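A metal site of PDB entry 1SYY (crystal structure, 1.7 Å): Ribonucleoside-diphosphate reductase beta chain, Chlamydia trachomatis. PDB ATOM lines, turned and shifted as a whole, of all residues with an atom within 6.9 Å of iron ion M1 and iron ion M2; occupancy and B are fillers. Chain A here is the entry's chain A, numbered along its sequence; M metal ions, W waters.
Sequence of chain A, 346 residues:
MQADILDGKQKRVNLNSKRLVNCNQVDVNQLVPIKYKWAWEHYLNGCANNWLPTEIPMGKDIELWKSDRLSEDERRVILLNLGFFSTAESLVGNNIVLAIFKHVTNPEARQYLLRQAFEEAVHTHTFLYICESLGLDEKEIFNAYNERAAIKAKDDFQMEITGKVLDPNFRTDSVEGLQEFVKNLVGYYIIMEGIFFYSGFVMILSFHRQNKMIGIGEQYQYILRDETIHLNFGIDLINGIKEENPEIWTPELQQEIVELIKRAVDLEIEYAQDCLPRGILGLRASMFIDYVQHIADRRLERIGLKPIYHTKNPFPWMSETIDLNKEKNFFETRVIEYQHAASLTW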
ATOM      1  N   PHE A  85      18.177  12.759 -20.180  1.00  0.00           N
ATOM      2  CA  PHE A  85      18.701  12.652 -18.800  1.00  0.00           C
ATOM      3  C   PHE A  85      19.900  11.736 -18.675  1.00  0.00           C
ATOM      4  O   PHE A  85      20.748  11.977 -17.827  1.00  0.00           O
ATOM      5  CB  PHE A  85      17.595  12.153 -17.833  1.00  0.00           C
ATOM      6  CG  PHE A  85      16.672  13.245 -17.326  1.00  0.00           C
ATOM      7  CD1 PHE A  85      15.578  13.646 -18.077  1.00  0.00           C
ATOM      8  CD2 PHE A  85      16.863  13.843 -16.086  1.00  0.00           C
ATOM      9  CE1 PHE A  85      14.681  14.615 -17.655  1.00  0.00           C
ATOM     10  CE2 PHE A  85      15.951  14.816 -15.638  1.00  0.00           C
ATOM     11  CZ  PHE A  85      14.845  15.194 -16.445  1.00  0.00           C
ATOM     12  N   ALA A  88      22.865  13.846 -19.302  1.00  0.00           N
ATOM     13  CA  ALA A  88      22.945  15.138 -18.628  1.00  0.00           C
ATOM     14  C   ALA A  88      23.341  14.976 -17.198  1.00  0.00           C
ATOM     15  O   ALA A  88      23.952  15.899 -16.627  1.00  0.00           O
ATOM     16  CB  ALA A  88      21.567  15.908 -18.658  1.00  0.00           C
ATOM     17  N   GLU A  89      22.980  13.859 -16.574  1.00  0.00           N
ATOM     18  CA  GLU A  89      23.397  13.669 -15.191  1.00  0.00           C
ATOM     19  C   GLU A  89      24.896  13.625 -15.151  1.00  0.00           C
ATOM     20  O   GLU A  89      25.468  14.208 -14.178  1.00  0.00           O
ATOM     21  CB  GLU A  89      22.892  12.325 -14.585  1.00  0.00           C
ATOM     22  CG  GLU A  89      21.359  12.193 -14.736  1.00  0.00           C
ATOM     23  CD  GLU A  89      20.588  13.119 -13.799  1.00  0.00           C
ATOM     24  OE1 GLU A  89      21.190  13.828 -12.948  1.00  0.00           O
ATOM     25  OE2 GLU A  89      19.358  13.143 -13.863  1.00  0.00           O
ATOM     26  N   VAL A  92      26.368  17.177 -15.386  1.00  0.00           N
ATOM     27  CA  VAL A  92      26.291  17.909 -14.110  1.00  0.00           C
ATOM     28  C   VAL A  92      27.340  17.397 -13.099  1.00  0.00           C
ATOM     29  O   VAL A  92      28.070  18.195 -12.489  1.00  0.00           O
ATOM     30  CB  VAL A  92      24.831  17.760 -13.474  1.00  0.00           C
ATOM     31  CG1 VAL A  92      24.754  18.585 -12.124  1.00  0.00           C
ATOM     32  CG2 VAL A  92      23.841  18.450 -14.466  1.00  0.00           C
ATOM     33  N   ILE A  96      30.473  19.473 -11.437  1.00  0.00           N
ATOM     34  CA  ILE A  96      30.718  19.744  -9.968  1.00  0.00           C
ATOM     35  C   ILE A  96      32.140  19.458  -9.614  1.00  0.00           C
ATOM     36  O   ILE A  96      32.785  20.210  -8.884  1.00  0.00           O
ATOM     37  CB  ILE A  96      29.808  18.739  -9.159  1.00  0.00           C
ATOM     38  CG1 ILE A  96      28.349  19.131  -9.246  1.00  0.00           C
ATOM     39  CG2 ILE A  96      30.252  18.802  -7.616  1.00  0.00           C
ATOM     40  CD1 ILE A  96      27.395  18.028  -8.823  1.00  0.00           C
ATOM     41  N   GLN A 116      26.327  15.911  -3.560  1.00  0.00           N
ATOM     42  CA  GLN A 116      25.595  16.198  -4.813  1.00  0.00           C
ATOM     43  C   GLN A 116      26.188  15.380  -5.946  1.00  0.00           C
ATOM     44  O   GLN A 116      25.415  14.785  -6.722  1.00  0.00           O
ATOM     45  CB  GLN A 116      25.669  17.686  -5.149  1.00  0.00           C
ATOM     46  CG  GLN A 116      24.685  18.023  -6.293  1.00  0.00           C
ATOM     47  CD  GLN A 116      24.882  19.402  -6.924  1.00  0.00           C
ATOM     48  OE1 GLN A 116      24.349  19.664  -8.074  1.00  0.00           O
ATOM     49  NE2 GLN A 116      25.645  20.251  -6.269  1.00  0.00           N
ATOM     50  N   GLU A 119      25.060  11.927  -5.717  1.00  0.00           N
ATOM     51  CA  GLU A 119      23.647  11.740  -6.149  1.00  0.00           C
ATOM     52  C   GLU A 119      23.560  11.753  -7.662  1.00  0.00           C
ATOM     53  O   GLU A 119      22.678  11.092  -8.217  1.00  0.00           O
ATOM     54  CB  GLU A 119      22.798  12.852  -5.575  1.00  0.00           C
ATOM     55  CG  GLU A 119      22.607  12.562  -4.005  1.00  0.00           C
ATOM     56  CD  GLU A 119      21.915  13.709  -3.248  1.00  0.00           C
ATOM     57  OE1 GLU A 119      21.691  14.824  -3.776  1.00  0.00           O
ATOM     58  OE2 GLU A 119      21.563  13.459  -2.100  1.00  0.00           O
ATOM     59  N   GLU A 120      24.391  12.544  -8.356  1.00  0.00           N
ATOM     60  CA  GLU A 120      24.276  12.508  -9.832  1.00  0.00           C
ATOM     61  C   GLU A 120      24.737  11.130 -10.345  1.00  0.00           C
ATOM     62  O   GLU A 120      24.215  10.664 -11.378  1.00  0.00           O
ATOM     63  CB  GLU A 120      25.149  13.598 -10.482  1.00  0.00           C
ATOM     64  CG  GLU A 120      24.847  15.050 -10.027  1.00  0.00           C
ATOM     65  CD  GLU A 120      23.427  15.511 -10.155  1.00  0.00           C
ATOM     66  OE1 GLU A 120      22.593  14.726 -10.666  1.00  0.00           O
ATOM     67  OE2 GLU A 120      23.149  16.698  -9.731  1.00  0.00           O
ATOM     68  N   ALA A 121      25.685  10.487  -9.675  1.00  0.00           N
ATOM     69  CA  ALA A 121      26.076   9.104 -10.060  1.00  0.00           C
ATOM     70  C   ALA A 121      24.853   8.162  -9.858  1.00  0.00           C
ATOM     71  O   ALA A 121      24.595   7.271 -10.696  1.00  0.00           O
ATOM     72  CB  ALA A 121      27.319   8.642  -9.185  1.00  0.00           C
ATOM     73  N   HIS A 123      21.788   9.104 -10.075  1.00  0.00           N
ATOM     74  CA  HIS A 123      20.838   9.389 -11.170  1.00  0.00           C
ATOM     75  C   HIS A 123      21.296   8.706 -12.442  1.00  0.00           C
ATOM     76  O   HIS A 123      20.463   8.202 -13.201  1.00  0.00           O
ATOM     77  CB  HIS A 123      20.743  10.914 -11.384  1.00  0.00           C
ATOM     78  CG  HIS A 123      20.173  11.603 -10.174  1.00  0.00           C
ATOM     79  ND1 HIS A 123      20.075  13.009 -10.048  1.00  0.00           N
ATOM     80  CD2 HIS A 123      19.720  11.060  -9.001  1.00  0.00           C
ATOM     81  CE1 HIS A 123      19.612  13.254  -8.838  1.00  0.00           C
ATOM     82  NE2 HIS A 123      19.397  12.113  -8.183  1.00  0.00           N
ATOM     83  N   THR A 124      22.602   8.698 -12.717  1.00  0.00           N
ATOM     84  CA  THR A 124      23.030   7.986 -13.976  1.00  0.00           C
ATOM     85  C   THR A 124      22.678   6.516 -13.901  1.00  0.00           C
ATOM     86  O   THR A 124      22.211   5.914 -14.909  1.00  0.00           O
ATOM     87  CB  THR A 124      24.545   8.118 -14.109  1.00  0.00           C
ATOM     88  OG1 THR A 124      24.872   9.520 -14.291  1.00  0.00           O
ATOM     89  CG2 THR A 124      25.139   7.320 -15.363  1.00  0.00           C
ATOM     90  N   PHE A 127      19.159   5.731 -14.929  1.00  0.00           N
ATOM     91  CA  PHE A 127      18.897   5.633 -16.346  1.00  0.00           C
ATOM     92  C   PHE A 127      19.426   4.321 -16.964  1.00  0.00           C
ATOM     93  O   PHE A 127      18.780   3.774 -17.858  1.00  0.00           O
ATOM     94  CB  PHE A 127      19.373   6.899 -17.077  1.00  0.00           C
ATOM     95  CG  PHE A 127      18.544   8.079 -16.658  1.00  0.00           C
ATOM     96  CD1 PHE A 127      17.145   8.135 -17.005  1.00  0.00           C
ATOM     97  CD2 PHE A 127      19.016   8.942 -15.743  1.00  0.00           C
ATOM     98  CE1 PHE A 127      16.319   9.035 -16.375  1.00  0.00           C
ATOM     99  CE2 PHE A 127      18.200   9.849 -15.120  1.00  0.00           C
ATOM    100  CZ  PHE A 127      16.841   9.903 -15.414  1.00  0.00           C
ATOM    101  N   TYR A 188      24.636  25.621 -14.667  1.00  0.00           N
ATOM    102  CA  TYR A 188      24.360  24.252 -14.204  1.00  0.00           C
ATOM    103  C   TYR A 188      23.232  24.199 -13.163  1.00  0.00           C
ATOM    104  O   TYR A 188      22.331  23.369 -13.270  1.00  0.00           O
ATOM    105  CB  TYR A 188      25.635  23.569 -13.689  1.00  0.00           C
ATOM    106  CG  TYR A 188      26.450  23.053 -14.857  1.00  0.00           C
ATOM    107  CD1 TYR A 188      26.280  21.719 -15.329  1.00  0.00           C
ATOM    108  CD2 TYR A 188      27.331  23.898 -15.523  1.00  0.00           C
ATOM    109  CE1 TYR A 188      27.017  21.277 -16.394  1.00  0.00           C
ATOM    110  CE2 TYR A 188      28.019  23.431 -16.682  1.00  0.00           C
ATOM    111  CZ  TYR A 188      27.849  22.143 -17.062  1.00  0.00           C
ATOM    112  OH  TYR A 188      28.550  21.704 -18.216  1.00  0.00           O
ATOM    113  N   TYR A 189      23.283  25.063 -12.153  1.00  0.00           N
ATOM    114  CA  TYR A 189      22.231  24.959 -11.121  1.00  0.00           C
ATOM    115  C   TYR A 189      20.929  25.534 -11.563  1.00  0.00           C
ATOM    116  O   TYR A 189      19.889  24.915 -11.399  1.00  0.00           O
ATOM    117  CB  TYR A 189      22.669  25.743  -9.837  1.00  0.00           C
ATOM    118  CG  TYR A 189      23.649  24.941  -9.025  1.00  0.00           C
ATOM    119  CD1 TYR A 189      23.221  23.798  -8.309  1.00  0.00           C
ATOM    120  CD2 TYR A 189      24.996  25.307  -9.003  1.00  0.00           C
ATOM    121  CE1 TYR A 189      24.178  23.069  -7.550  1.00  0.00           C
ATOM    122  CE2 TYR A 189      25.955  24.565  -8.284  1.00  0.00           C
ATOM    123  CZ  TYR A 189      25.522  23.463  -7.557  1.00  0.00           C
ATOM    124  OH  TYR A 189      26.496  22.760  -6.890  1.00  0.00           O
ATOM    125  N   GLU A 193      19.782  22.165 -14.024  1.00  0.00           N
ATOM    126  CA  GLU A 193      18.990  21.513 -12.994  1.00  0.00           C
ATOM    127  C   GLU A 193      17.684  22.173 -12.731  1.00  0.00           C
ATOM    128  O   GLU A 193      16.686  21.523 -12.486  1.00  0.00           O
ATOM    129  CB  GLU A 193      19.803  21.449 -11.670  1.00  0.00           C
ATOM    130  CG  GLU A 193      21.034  20.483 -11.929  1.00  0.00           C
ATOM    131  CD  GLU A 193      22.045  20.414 -10.755  1.00  0.00           C
ATOM    132  OE1 GLU A 193      22.766  21.375 -10.449  1.00  0.00           O
ATOM    133  OE2 GLU A 193      22.165  19.384 -10.161  1.00  0.00           O
ATOM    134  N   PHE A 197      15.748  20.275 -16.394  1.00  0.00           N
ATOM    135  CA  PHE A 197      15.293  18.976 -15.755  1.00  0.00           C
ATOM    136  C   PHE A 197      13.866  19.071 -15.279  1.00  0.00           C
ATOM    137  O   PHE A 197      13.090  18.127 -15.440  1.00  0.00           O
ATOM    138  CB  PHE A 197      16.131  18.626 -14.570  1.00  0.00           C
ATOM    139  CG  PHE A 197      17.545  18.195 -14.905  1.00  0.00           C
ATOM    140  CD1 PHE A 197      17.942  17.924 -16.192  1.00  0.00           C
ATOM    141  CD2 PHE A 197      18.464  17.937 -13.879  1.00  0.00           C
ATOM    142  CE1 PHE A 197      19.179  17.417 -16.452  1.00  0.00           C
ATOM    143  CE2 PHE A 197      19.689  17.426 -14.145  1.00  0.00           C
ATOM    144  CZ  PHE A 197      20.067  17.165 -15.435  1.00  0.00           C
ATOM    145  N   PHE A 201      10.672  16.555 -15.788  1.00  0.00           N
ATOM    146  CA  PHE A 201       9.947  15.969 -14.635  1.00  0.00           C
ATOM    147  C   PHE A 201       8.465  16.076 -14.839  1.00  0.00           C
ATOM    148  O   PHE A 201       7.734  15.156 -14.508  1.00  0.00           O
ATOM    149  CB  PHE A 201      10.272  16.757 -13.303  1.00  0.00           C
ATOM    150  CG  PHE A 201      11.705  16.668 -12.859  1.00  0.00           C
ATOM    151  CD1 PHE A 201      12.472  15.544 -13.071  1.00  0.00           C
ATOM    152  CD2 PHE A 201      12.269  17.703 -12.144  1.00  0.00           C
ATOM    153  CE1 PHE A 201      13.800  15.452 -12.590  1.00  0.00           C
ATOM    154  CE2 PHE A 201      13.612  17.609 -11.629  1.00  0.00           C
ATOM    155  CZ  PHE A 201      14.356  16.493 -11.865  1.00  0.00           C
ATOM    156  N   ILE A 223      14.419  11.515  -7.957  1.00  0.00           N
ATOM    157  CA  ILE A 223      15.372  12.484  -8.560  1.00  0.00           C
ATOM    158  C   ILE A 223      14.905  13.915  -8.284  1.00  0.00           C
ATOM    159  O   ILE A 223      15.720  14.772  -7.922  1.00  0.00           O
ATOM    160  CB  ILE A 223      15.538  12.257 -10.089  1.00  0.00           C
ATOM    161  CG1 ILE A 223      16.128  10.899 -10.271  1.00  0.00           C
ATOM    162  CG2 ILE A 223      16.308  13.362 -10.749  1.00  0.00           C
ATOM    163  CD1 ILE A 223      16.134  10.411 -11.780  1.00  0.00           C
ATOM    164  N   ASP A 226      15.841  15.030  -4.856  1.00  0.00           N
ATOM    165  CA  ASP A 226      17.268  15.447  -4.811  1.00  0.00           C
ATOM    166  C   ASP A 226      17.461  16.805  -5.513  1.00  0.00           C
ATOM    167  O   ASP A 226      18.123  17.672  -4.979  1.00  0.00           O
ATOM    168  CB  ASP A 226      18.205  14.447  -5.512  1.00  0.00           C
ATOM    169  CG  ASP A 226      18.228  13.079  -4.852  1.00  0.00           C
ATOM    170  OD1 ASP A 226      18.033  12.984  -3.632  1.00  0.00           O
ATOM    171  OD2 ASP A 226      18.518  12.095  -5.597  1.00  0.00           O
ATOM    172  N   GLU A 227      16.920  16.972  -6.721  1.00  0.00           N
ATOM    173  CA  GLU A 227      17.146  18.196  -7.527  1.00  0.00           C
ATOM    174  C   GLU A 227      16.691  19.438  -6.798  1.00  0.00           C
ATOM    175  O   GLU A 227      17.247  20.545  -6.991  1.00  0.00           O
ATOM    176  CB  GLU A 227      16.372  18.110  -8.849  1.00  0.00           C
ATOM    177  CG  GLU A 227      16.986  19.011  -9.850  1.00  0.00           C
ATOM    178  CD  GLU A 227      18.279  18.286 -10.274  1.00  0.00           C
ATOM    179  OE1 GLU A 227      18.126  17.352 -11.071  1.00  0.00           O
ATOM    180  OE2 GLU A 227      19.407  18.587  -9.778  1.00  0.00           O
ATOM    181  N   HIS A 230      19.535  20.283  -4.756  1.00  0.00           N
ATOM    182  CA  HIS A 230      20.635  20.787  -5.582  1.00  0.00           C
ATOM    183  C   HIS A 230      20.442  22.272  -5.988  1.00  0.00           C
ATOM    184  O   HIS A 230      21.357  23.085  -5.909  1.00  0.00           O
ATOM    185  CB  HIS A 230      20.753  19.966  -6.871  1.00  0.00           C
ATOM    186  CG  HIS A 230      21.082  18.518  -6.638  1.00  0.00           C
ATOM    187  ND1 HIS A 230      21.308  17.629  -7.681  1.00  0.00           N
ATOM    188  CD2 HIS A 230      21.251  17.823  -5.508  1.00  0.00           C
ATOM    189  CE1 HIS A 230      21.573  16.433  -7.172  1.00  0.00           C
ATOM    190  NE2 HIS A 230      21.543  16.522  -5.852  1.00  0.00           N
ATOM    191  N   LEU A 231      19.229  22.576  -6.436  1.00  0.00           N
ATOM    192  CA  LEU A 231      18.898  23.931  -6.874  1.00  0.00           C
ATOM    193  C   LEU A 231      19.008  24.894  -5.688  1.00  0.00           C
ATOM    194  O   LEU A 231      19.547  25.990  -5.859  1.00  0.00           O
ATOM    195  CB  LEU A 231      17.481  23.906  -7.407  1.00  0.00           C
ATOM    196  CG  LEU A 231      16.916  25.288  -7.737  1.00  0.00           C
ATOM    197  CD1 LEU A 231      17.722  25.996  -8.829  1.00  0.00           C
ATOM    198  CD2 LEU A 231      15.444  25.071  -8.198  1.00  0.00           C
HETATM  199 FE    FE M   1      21.277  17.634  -9.815  1.00  0.00          FE
HETATM  200 FE    FE M   2      20.655  14.730 -11.340  1.00  0.00          FE
HETATM  201  O   HOH W   1      19.909  16.016  -9.901  1.00  0.00           O
HETATM  202  O   HOH W   2      18.767  14.932 -12.113  1.00  0.00           O
HETATM  203  O   HOH W   3      21.142  16.825 -11.872  1.00  0.00           O
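Iron ion M1 is bound by OE2 of Glu 193, 2.0 Å away.
Iron ion M1 is bound by OE2 of Glu 120 (2.1 Å).
OE2 of Glu 227 binds iron ion M1, 2.1 Å away.
Water W1 binds iron ion M1.
A ring nitrogen (ND1) of His 230 is bound to iron ion M1, 2.1 Å away.
Iron ion M1 is bound by water W3.
Iron ion M1 has six donor atoms within binding distance.
Iron ion M2 is bound by the side-chain carboxylate of Glu 89, water W2, the side-chain carboxylate of Glu 120, water W1, water W3 and a ring nitrogen (ND1) of His 123.
Four residues have an atom within 4 Å of iron ion M2: Glu 89, Glu 120, His 123 and Glu 227.
OE1 of Glu 193 lies close to OE1 of Gln 116 (3.3 Å).
The backbone NH (N) of Glu 193 is in hydrogen-bond range of the backbone carbonyl oxygen (O) of Tyr 188 (2.9 Å).
The backbone carbonyl oxygen (O) of Glu 120 sits at hydrogen-bond distance from the side-chain hydroxyl (OG1) of Thr 124.
NE2 of His 230 lies within hydrogen-bond range of OE1 of Glu 119.
A ring nitrogen (NE2) of His 123 lies close to the backbone carbonyl oxygen (O) of Glu 119 (3.4 Å).
A ring nitrogen (NE2) of His 123 is in hydrogen-bond range of the side-chain carboxylate (OD2) of Asp 226, at 2.7 Å.
Water W2 bridges OE2 of Glu 89 (2.6 Å) and OE1 of Glu 227 (2.7 Å).
Within 4 Å of iron ion M1: Glu 120, Glu 193, Glu 227 and His 230.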
